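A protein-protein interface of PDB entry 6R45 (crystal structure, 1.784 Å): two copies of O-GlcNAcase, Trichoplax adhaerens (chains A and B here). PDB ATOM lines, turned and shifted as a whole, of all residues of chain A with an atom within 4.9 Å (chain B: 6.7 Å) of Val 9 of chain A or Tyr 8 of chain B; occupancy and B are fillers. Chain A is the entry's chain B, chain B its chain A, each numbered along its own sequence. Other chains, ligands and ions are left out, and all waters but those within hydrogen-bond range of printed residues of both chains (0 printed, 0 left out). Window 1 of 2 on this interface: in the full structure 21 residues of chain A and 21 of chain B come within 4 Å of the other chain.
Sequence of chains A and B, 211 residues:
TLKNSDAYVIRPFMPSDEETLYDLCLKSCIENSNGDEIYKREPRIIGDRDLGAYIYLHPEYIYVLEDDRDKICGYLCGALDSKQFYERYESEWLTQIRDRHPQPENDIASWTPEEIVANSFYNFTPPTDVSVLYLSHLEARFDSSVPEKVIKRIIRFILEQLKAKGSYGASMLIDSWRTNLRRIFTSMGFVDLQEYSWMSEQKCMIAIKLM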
ATOM      1  N   ALA A   7     -23.678 -19.564  -1.313  1.00  0.00           N
ATOM      2  CA  ALA A   7     -22.431 -18.875  -1.650  1.00  0.00           C
ATOM      3  C   ALA A   7     -22.075 -17.977  -0.479  1.00  0.00           C
ATOM      4  O   ALA A   7     -22.758 -16.927  -0.267  1.00  0.00           O
ATOM      5  CB  ALA A   7     -22.587 -18.066  -2.920  1.00  0.00           C
ATOM      6  N   TYR A   8     -20.988 -18.298   0.199  1.00  0.00           N
ATOM      7  CA  TYR A   8     -20.343 -17.356   1.135  1.00  0.00           C
ATOM      8  C   TYR A   8     -19.351 -16.480   0.378  1.00  0.00           C
ATOM      9  O   TYR A   8     -18.683 -16.908  -0.571  1.00  0.00           O
ATOM     10  CB  TYR A   8     -19.664 -18.077   2.291  1.00  0.00           C
ATOM     11  CG  TYR A   8     -20.631 -18.754   3.220  1.00  0.00           C
ATOM     12  CD1 TYR A   8     -21.352 -19.873   2.819  1.00  0.00           C
ATOM     13  CD2 TYR A   8     -20.859 -18.240   4.487  1.00  0.00           C
ATOM     14  CE1 TYR A   8     -22.265 -20.483   3.666  1.00  0.00           C
ATOM     15  CE2 TYR A   8     -21.771 -18.834   5.339  1.00  0.00           C
ATOM     16  CZ  TYR A   8     -22.471 -19.951   4.925  1.00  0.00           C
ATOM     17  OH  TYR A   8     -23.347 -20.508   5.801  1.00  0.00           O
ATOM     18  N   VAL A   9     -19.256 -15.234   0.801  1.00  0.00           N
ATOM     19  CA  VAL A   9     -18.280 -14.288   0.205  1.00  0.00           C
ATOM     20  C   VAL A   9     -17.327 -13.828   1.298  1.00  0.00           C
ATOM     21  O   VAL A   9     -17.774 -13.380   2.358  1.00  0.00           O
ATOM     22  CB  VAL A   9     -18.948 -13.086  -0.482  1.00  0.00           C
ATOM     23  CG1 VAL A   9     -17.911 -12.055  -0.885  1.00  0.00           C
ATOM     24  CG2 VAL A   9     -19.752 -13.554  -1.680  1.00  0.00           C
ATOM     25  N   ILE A  10     -16.044 -13.888   0.984  1.00  0.00           N
ATOM     26  CA  ILE A  10     -14.946 -13.309   1.782  1.00  0.00           C
ATOM     27  C   ILE A  10     -14.448 -12.074   1.034  1.00  0.00           C
ATOM     28  O   ILE A  10     -14.014 -12.198  -0.115  1.00  0.00           O
ATOM     29  CB  ILE A  10     -13.841 -14.372   1.958  1.00  0.00           C
ATOM     30  CG1 ILE A  10     -14.383 -15.609   2.681  1.00  0.00           C
ATOM     31  CG2 ILE A  10     -12.607 -13.781   2.612  1.00  0.00           C
ATOM     32  CD1 ILE A  10     -13.672 -16.873   2.302  1.00  0.00           C
ATOM     33  N   ARG A  11     -14.486 -10.912   1.662  1.00  0.00           N
ATOM     34  CA  ARG A  11     -14.173  -9.653   0.948  1.00  0.00           C
ATOM     35  C   ARG A  11     -13.443  -8.744   1.910  1.00  0.00           C
ATOM     36  O   ARG A  11     -13.522  -8.942   3.117  1.00  0.00           O
ATOM     37  CB  ARG A  11     -15.460  -9.025   0.423  1.00  0.00           C
ATOM     38  CG  ARG A  11     -16.462  -8.689   1.524  1.00  0.00           C
ATOM     39  CD  ARG A  11     -17.255  -7.475   1.144  1.00  0.00           C
ATOM     40  NE  ARG A  11     -18.297  -7.241   2.109  1.00  0.00           N
ATOM     41  CZ  ARG A  11     -18.222  -6.407   3.133  1.00  0.00           C
ATOM     42  NH1 ARG A  11     -17.131  -5.713   3.389  1.00  0.00           N
ATOM     43  NH2 ARG A  11     -19.265  -6.296   3.926  1.00  0.00           N
ATOM     44  N   VAL A  64     -13.935  -9.782   5.735  1.00  0.00           N
ATOM     45  CA  VAL A  64     -15.287  -9.955   6.286  1.00  0.00           C
ATOM     46  C   VAL A  64     -15.902 -11.153   5.576  1.00  0.00           C
ATOM     47  O   VAL A  64     -15.694 -11.264   4.390  1.00  0.00           O
ATOM     48  CB  VAL A  64     -16.072  -8.655   6.065  1.00  0.00           C
ATOM     49  CG1 VAL A  64     -17.531  -8.820   6.374  1.00  0.00           C
ATOM     50  CG2 VAL A  64     -15.428  -7.527   6.859  1.00  0.00           C
ATOM     51  N   LEU A  65     -16.659 -11.963   6.309  1.00  0.00           N
ATOM     52  CA  LEU A  65     -17.348 -13.159   5.802  1.00  0.00           C
ATOM     53  C   LEU A  65     -18.853 -12.879   5.782  1.00  0.00           C
ATOM     54  O   LEU A  65     -19.401 -12.526   6.849  1.00  0.00           O
ATOM     55  CB  LEU A  65     -17.030 -14.349   6.702  1.00  0.00           C
ATOM     56  CG  LEU A  65     -17.770 -15.625   6.299  1.00  0.00           C
ATOM     57  CD1 LEU A  65     -17.284 -16.098   4.947  1.00  0.00           C
ATOM     58  CD2 LEU A  65     -17.632 -16.700   7.360  1.00  0.00           C
ATOM     59  N   GLU A  66     -19.472 -13.082   4.618  1.00  0.00           N
ATOM     60  CA  GLU A  66     -20.929 -12.944   4.402  1.00  0.00           C
ATOM     61  C   GLU A  66     -21.489 -14.294   4.009  1.00  0.00           C
ATOM     62  O   GLU A  66     -20.854 -15.038   3.259  1.00  0.00           O
ATOM     63  CB  GLU A  66     -21.241 -11.948   3.295  1.00  0.00           C
ATOM     64  CG  GLU A  66     -20.850 -10.531   3.621  1.00  0.00           C
ATOM     65  CD  GLU A  66     -20.806  -9.617   2.410  1.00  0.00           C
ATOM     66  OE1 GLU A  66     -20.763 -10.141   1.251  1.00  0.00           O
ATOM     67  OE2 GLU A  66     -20.844  -8.390   2.625  1.00  0.00           O
ATOM     68  N   ASP B   6     -20.322 -23.094  -0.785  1.00  0.00           N
ATOM     69  CA  ASP B   6     -19.112 -22.664  -1.513  1.00  0.00           C
ATOM     70  C   ASP B   6     -18.712 -21.317  -0.933  1.00  0.00           C
ATOM     71  O   ASP B   6     -19.608 -20.511  -0.579  1.00  0.00           O
ATOM     72  CB  ASP B   6     -19.341 -22.626  -3.022  1.00  0.00           C
ATOM     73  CG  ASP B   6     -19.683 -24.008  -3.535  1.00  0.00           C
ATOM     74  OD1 ASP B   6     -19.246 -24.978  -2.888  1.00  0.00           O
ATOM     75  OD2 ASP B   6     -20.400 -24.096  -4.539  1.00  0.00           O
ATOM     76  N   ALA B   7     -17.424 -21.075  -0.807  1.00  0.00           N
ATOM     77  CA  ALA B   7     -16.966 -19.795  -0.222  1.00  0.00           C
ATOM     78  C   ALA B   7     -16.020 -19.136  -1.221  1.00  0.00           C
ATOM     79  O   ALA B   7     -14.951 -19.704  -1.509  1.00  0.00           O
ATOM     80  CB  ALA B   7     -16.340 -20.043   1.121  1.00  0.00           C
ATOM     81  N   TYR B   8     -16.464 -18.018  -1.771  1.00  0.00           N
ATOM     82  CA  TYR B   8     -15.736 -17.204  -2.760  1.00  0.00           C
ATOM     83  C   TYR B   8     -14.934 -16.142  -2.015  1.00  0.00           C
ATOM     84  O   TYR B   8     -15.342 -15.648  -0.982  1.00  0.00           O
ATOM     85  CB  TYR B   8     -16.704 -16.570  -3.767  1.00  0.00           C
ATOM     86  CG  TYR B   8     -17.417 -17.582  -4.627  1.00  0.00           C
ATOM     87  CD1 TYR B   8     -18.503 -18.298  -4.121  1.00  0.00           C
ATOM     88  CD2 TYR B   8     -16.975 -17.889  -5.904  1.00  0.00           C
ATOM     89  CE1 TYR B   8     -19.127 -19.274  -4.875  1.00  0.00           C
ATOM     90  CE2 TYR B   8     -17.626 -18.826  -6.694  1.00  0.00           C
ATOM     91  CZ  TYR B   8     -18.705 -19.520  -6.166  1.00  0.00           C
ATOM     92  OH  TYR B   8     -19.317 -20.515  -6.880  1.00  0.00           O
ATOM     93  N   VAL B   9     -13.795 -15.804  -2.585  1.00  0.00           N
ATOM     94  CA  VAL B   9     -12.928 -14.706  -2.124  1.00  0.00           C
ATOM     95  C   VAL B   9     -12.858 -13.653  -3.217  1.00  0.00           C
ATOM     96  O   VAL B   9     -12.482 -13.970  -4.369  1.00  0.00           O
ATOM     97  CB  VAL B   9     -11.522 -15.204  -1.772  1.00  0.00           C
ATOM     98  CG1 VAL B   9     -10.674 -14.039  -1.308  1.00  0.00           C
ATOM     99  CG2 VAL B   9     -11.545 -16.326  -0.738  1.00  0.00           C
ATOM    100  N   ILE B  10     -13.137 -12.418  -2.844  1.00  0.00           N
ATOM    101  CA  ILE B  10     -12.771 -11.266  -3.678  1.00  0.00           C
ATOM    102  C   ILE B  10     -11.606 -10.583  -2.968  1.00  0.00           C
ATOM    103  O   ILE B  10     -11.661 -10.301  -1.781  1.00  0.00           O
ATOM    104  CB  ILE B  10     -13.992 -10.369  -3.987  1.00  0.00           C
ATOM    105  CG1 ILE B  10     -13.610  -9.242  -4.942  1.00  0.00           C
ATOM    106  CG2 ILE B  10     -14.682  -9.863  -2.738  1.00  0.00           C
ATOM    107  CD1 ILE B  10     -13.355  -9.732  -6.381  1.00  0.00           C
ATOM    108  N   LEU B  65     -11.453 -12.715  -8.203  1.00  0.00           N
ATOM    109  CA  LEU B  65     -12.412 -13.621  -7.551  1.00  0.00           C
ATOM    110  C   LEU B  65     -11.827 -15.030  -7.547  1.00  0.00           C
ATOM    111  O   LEU B  65     -11.498 -15.535  -8.644  1.00  0.00           O
ATOM    112  CB  LEU B  65     -13.710 -13.558  -8.358  1.00  0.00           C
ATOM    113  CG  LEU B  65     -14.849 -14.411  -7.820  1.00  0.00           C
ATOM    114  CD1 LEU B  65     -15.262 -13.883  -6.449  1.00  0.00           C
ATOM    115  CD2 LEU B  65     -16.025 -14.388  -8.813  1.00  0.00           C
ATOM    116  N   GLU B  66     -11.739 -15.651  -6.369  1.00  0.00           N
ATOM    117  CA  GLU B  66     -11.378 -17.079  -6.192  1.00  0.00           C
ATOM    118  C   GLU B  66     -12.613 -17.890  -5.802  1.00  0.00           C
ATOM    119  O   GLU B  66     -13.398 -17.402  -4.960  1.00  0.00           O
ATOM    120  CB  GLU B  66     -10.374 -17.268  -5.064  1.00  0.00           C
ATOM    121  CG  GLU B  66      -9.018 -16.661  -5.315  1.00  0.00           C
ATOM    122  CD  GLU B  66      -8.063 -16.900  -4.156  1.00  0.00           C
ATOM    123  OE1 GLU B  66      -8.130 -18.013  -3.602  1.00  0.00           O
ATOM    124  OE2 GLU B  66      -7.268 -15.975  -3.810  1.00  0.00           O
ATOM    125  N   ASP B  67     -12.775 -19.079  -6.375  1.00  0.00           N
ATOM    126  CA  ASP B  67     -13.867 -20.013  -5.995  1.00  0.00           C
ATOM    127  C   ASP B  67     -13.473 -20.801  -4.753  1.00  0.00           C
ATOM    128  O   ASP B  67     -12.402 -20.520  -4.192  1.00  0.00           O
ATOM    129  CB  ASP B  67     -14.268 -20.900  -7.171  1.00  0.00           C
ATOM    130  CG  ASP B  67     -13.249 -21.972  -7.511  1.00  0.00           C
ATOM    131  OD1 ASP B  67     -12.297 -22.163  -6.730  1.00  0.00           O
ATOM    132  OD2 ASP B  67     -13.411 -22.562  -8.574  1.00  0.00           O
ATOM    133  N   ASP B  68     -14.304 -21.786  -4.383  1.00  0.00           N
ATOM    134  CA  ASP B  68     -14.212 -22.548  -3.112  1.00  0.00           C
ATOM    135  C   ASP B  68     -12.912 -23.361  -3.048  1.00  0.00           C
ATOM    136  O   ASP B  68     -12.440 -23.615  -1.920  1.00  0.00           O
ATOM    137  CB  ASP B  68     -15.423 -23.458  -2.950  1.00  0.00           C
ATOM    138  CG  ASP B  68     -15.444 -24.067  -1.583  1.00  0.00           C
ATOM    139  OD1 ASP B  68     -15.592 -23.295  -0.609  1.00  0.00           O
ATOM    140  OD2 ASP B  68     -15.219 -25.292  -1.492  1.00  0.00           O
ATOM    141  N   CYS B  73     -11.574 -17.288 -11.003  1.00  0.00           N
ATOM    142  CA  CYS B  73     -12.731 -17.473 -11.915  1.00  0.00           C
ATOM    143  C   CYS B  73     -13.318 -16.108 -12.326  1.00  0.00           C
ATOM    144  O   CYS B  73     -14.365 -16.054 -12.970  1.00  0.00           O
ATOM    145  CB  CYS B  73     -13.760 -18.362 -11.235  1.00  0.00           C
ATOM    146  SG  CYS B  73     -14.311 -17.657  -9.670  1.00  0.00           S
ATOM    147  N   SER B 145     -18.339 -20.755 -14.722  1.00  0.00           N
ATOM    148  CA  SER B 145     -18.586 -21.459 -13.447  1.00  0.00           C
ATOM    149  C   SER B 145     -19.243 -20.499 -12.431  1.00  0.00           C
ATOM    150  O   SER B 145     -19.934 -20.975 -11.538  1.00  0.00           O
ATOM    151  CB  SER B 145     -17.304 -22.070 -12.954  1.00  0.00           C
ATOM    152  OG  SER B 145     -16.449 -21.124 -12.314  1.00  0.00           O
ATOM    153  N   VAL B 146     -19.099 -19.180 -12.576  1.00  0.00           N
ATOM    154  CA  VAL B 146     -19.474 -18.242 -11.471  1.00  0.00           C
ATOM    155  C   VAL B 146     -20.996 -18.090 -11.397  1.00  0.00           C
ATOM    156  O   VAL B 146     -21.643 -17.703 -12.373  1.00  0.00           O
ATOM    157  CB  VAL B 146     -18.779 -16.878 -11.586  1.00  0.00           C
ATOM    158  CG1 VAL B 146     -19.060 -16.040 -10.335  1.00  0.00           C
ATOM    159  CG2 VAL B 146     -17.275 -17.020 -11.775  1.00  0.00           C
ATOM    160  N   PRO B 147     -21.628 -18.405 -10.255  1.00  0.00           N
ATOM    161  CA  PRO B 147     -23.068 -18.188 -10.095  1.00  0.00           C
ATOM    162  C   PRO B 147     -23.417 -16.712 -10.319  1.00  0.00           C
ATOM    163  O   PRO B 147     -22.724 -15.839  -9.880  1.00  0.00           O
ATOM    164  CB  PRO B 147     -23.360 -18.566  -8.643  1.00  0.00           C
ATOM    165  CG  PRO B 147     -22.244 -19.518  -8.265  1.00  0.00           C
ATOM    166  CD  PRO B 147     -21.049 -19.040  -9.067  1.00  0.00           C
ATOM    167  N   LYS B 149     -25.631 -14.988  -8.807  1.00  0.00           N
ATOM    168  CA  LYS B 149     -25.831 -14.331  -7.479  1.00  0.00           C
ATOM    169  C   LYS B 149     -24.489 -13.871  -6.937  1.00  0.00           C
ATOM    170  O   LYS B 149     -24.415 -12.788  -6.351  1.00  0.00           O
ATOM    171  CB  LYS B 149     -26.545 -15.215  -6.455  1.00  0.00           C
ATOM    172  CG  LYS B 149     -25.891 -16.551  -6.136  1.00  0.00           C
ATOM    173  CD  LYS B 149     -26.826 -17.411  -5.254  1.00  0.00           C
ATOM    174  CE  LYS B 149     -26.222 -18.720  -4.789  1.00  0.00           C
ATOM    175  NZ  LYS B 149     -27.087 -19.291  -3.738  1.00  0.00           N
ATOM    176  N   VAL B 150     -23.426 -14.601  -7.261  1.00  0.00           N
ATOM    177  CA  VAL B 150     -22.075 -14.184  -6.818  1.00  0.00           C
ATOM    178  C   VAL B 150     -21.622 -12.981  -7.647  1.00  0.00           C
ATOM    179  O   VAL B 150     -21.159 -12.011  -7.038  1.00  0.00           O
ATOM    180  CB  VAL B 150     -21.116 -15.381  -6.881  1.00  0.00           C
ATOM    181  CG1 VAL B 150     -19.684 -14.949  -6.699  1.00  0.00           C
ATOM    182  CG2 VAL B 150     -21.504 -16.438  -5.847  1.00  0.00           C
ATOM    183  N   ARG B 153     -23.240  -9.867  -6.338  1.00  0.00           N
ATOM    184  CA  ARG B 153     -22.714  -9.491  -5.014  1.00  0.00           C
ATOM    185  C   ARG B 153     -21.354  -8.830  -5.220  1.00  0.00           C
ATOM    186  O   ARG B 153     -21.079  -7.808  -4.565  1.00  0.00           O
ATOM    187  CB  ARG B 153     -22.726 -10.710  -4.101  1.00  0.00           C
ATOM    188  CG  ARG B 153     -24.119 -11.010  -3.573  1.00  0.00           C
ATOM    189  CD  ARG B 153     -24.202 -12.293  -2.796  1.00  0.00           C
ATOM    190  NE  ARG B 153     -23.531 -12.105  -1.525  1.00  0.00           N
ATOM    191  CZ  ARG B 153     -23.205 -13.092  -0.706  1.00  0.00           C
ATOM    192  NH1 ARG B 153     -23.521 -14.332  -1.030  1.00  0.00           N
ATOM    193  NH2 ARG B 153     -22.582 -12.816   0.431  1.00  0.00           N
ATOM    194  N   ILE B 154     -20.557  -9.380  -6.125  1.00  0.00           N
ATOM    195  CA  ILE B 154     -19.175  -8.882  -6.371  1.00  0.00           C
ATOM    196  C   ILE B 154     -19.215  -7.540  -7.079  1.00  0.00           C
ATOM    197  O   ILE B 154     -18.437  -6.624  -6.689  1.00  0.00           O
ATOM    198  CB  ILE B 154     -18.344  -9.925  -7.130  1.00  0.00           C
ATOM    199  CG1 ILE B 154     -18.236 -11.214  -6.312  1.00  0.00           C
ATOM    200  CG2 ILE B 154     -16.987  -9.352  -7.471  1.00  0.00           C
ATOM    201  CD1 ILE B 154     -17.864 -10.988  -4.865  1.00  0.00           C
ATOM    202  N   PHE B 157     -20.078  -5.007  -4.455  1.00  0.00           N
ATOM    203  CA  PHE B 157     -18.893  -4.719  -3.600  1.00  0.00           C
ATOM    204  C   PHE B 157     -18.052  -3.601  -4.238  1.00  0.00           C
ATOM    205  O   PHE B 157     -17.717  -2.584  -3.567  1.00  0.00           O
ATOM    206  CB  PHE B 157     -18.070  -5.976  -3.337  1.00  0.00           C
ATOM    207  CG  PHE B 157     -16.698  -5.650  -2.790  1.00  0.00           C
ATOM    208  CD1 PHE B 157     -16.564  -5.152  -1.503  1.00  0.00           C
ATOM    209  CD2 PHE B 157     -15.567  -5.735  -3.592  1.00  0.00           C
ATOM    210  CE1 PHE B 157     -15.315  -4.802  -1.008  1.00  0.00           C
ATOM    211  CE2 PHE B 157     -14.323  -5.387  -3.094  1.00  0.00           C
ATOM    212  CZ  PHE B 157     -14.202  -4.909  -1.807  1.00  0.00           C
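N of Ile 10 of chain A sits at hydrogen-bond distance from O of Tyr 8 of chain B, at 2.7 Å.
O of Asp 6 of chain B lies within hydrogen-bond range of N of Tyr 8 of chain A.
The backbone NH (N) of Ile 10 of chain B sits at hydrogen-bond distance from the backbone carbonyl oxygen (O) of Ile 10 of chain A.
The guanidinium group (NH2) of Arg 153 of chain B lies within salt-bridge range of the side-chain carboxylate (OE1) of Glu 66 of chain A, at 3.3 Å.
The guanidinium group (NH1) of Arg 153 of chain B is in hydrogen-bond range of the backbone carbonyl oxygen (O) of Ala 7 of chain A.
The backbone NH (N) of Tyr 8 of chain B is in hydrogen-bond range of the backbone carbonyl oxygen (O) of Tyr 8 of chain A (2.8 Å).
O of Arg 11 of chain A lies within hydrogen-bond range of N of Val 64 of chain A, 2.8 Å away.
The backbone NH (N) of Glu 66 of chain A is in hydrogen-bond range of the backbone carbonyl oxygen (O) of Val 9 of chain A (2.8 Å).
NE of Arg 11 of chain A is in salt-bridge range of OE2 of Glu 66 of chain A (2.8 Å).
The backbone NH (N) of Glu 66 of chain B is in hydrogen-bond range of the backbone carbonyl oxygen (O) of Val 9 of chain B (2.7 Å).
The backbone NH (N) of Ala 7 of chain B is in hydrogen-bond range of the side-chain carboxylate (OD1) of Asp 68 of chain B, 2.9 Å away.
Among the printed residues, pairs that only touch across the chains: Ala 7 of chain A with Asp 6 of chain B (3.4 Å), Ala 7 of chain A with Val 150 of chain B (3.5 Å), Tyr 8 of chain A with Ala 7 of chain B (3.4 Å), Val 9 of chain A with Tyr 8 of chain B (3.4 Å), Val 9 of chain A with Arg 153 of chain B (3.6 Å), Ile 10 of chain A with Val 9 of chain B (3.4 Å), Arg 11 of chain A with Ile 10 of chain B (3.4 Å) and Arg 11 of chain A with Phe 157 of chain B (3.6 Å).
Of the printed residues of chain B, Val 9 of chain A touches Tyr 8 and Arg 153.
Of the printed residues of chain A, Asp 6 of chain B touches Ala 7 (3.4 Å) and Tyr 8 (2.7 Å).
Printed residues of chain A within 4 Å of Val 9 of chain B: Ile 10.
Printed residues of chain A within 4 Å of Phe 157 of chain B: Arg 11 (3.6 Å).
The nearest residue of chain B that does not touch Val 9 of chain A is Ile 154 of chain B (4.1 Å).
The nearest printed residue of chain A that does not touch Val 9 of chain B is Tyr 8 of chain A (5.4 Å).
Of the 8 printed residues of chain A, 6 touch a printed residue of chain B.
Hydrophobic or aromatic side chains of chain A within 4 Å of the printed part of chain B: Ala 7, Tyr 8, Val 9 and Ile 10.
Among the printed residues, Asp or Glu carboxylates within 4 Å of a Lys or Arg side-chain nitrogen of the other chain: Glu 66 of chain A with Arg 153 of chain B (3.3 Å).
Tyr 8 of chain A touches Ala 7 of chain B, but with the chains exchanged Ala 7 of chain A does not touch Tyr 8 of chain B (4.2 Å).
Tyr 8 of chain A touches its own counterpart, Tyr 8 of chain B.
Val 9 of chain A touches Tyr 8 of chain B, but with the chains exchanged Tyr 8 of chain A does not touch Val 9 of chain B (5.4 Å).
Ile 10 of chain A touches Val 9 of chain B, but with the chains exchanged Val 9 of chain A does not touch Ile 10 of chain B (4.3 Å).
6 positions are printed for both chains.
Of the 14 pairs that touch across the chains among the printed residues, 2 have their exchanged pair printed and touching as well.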
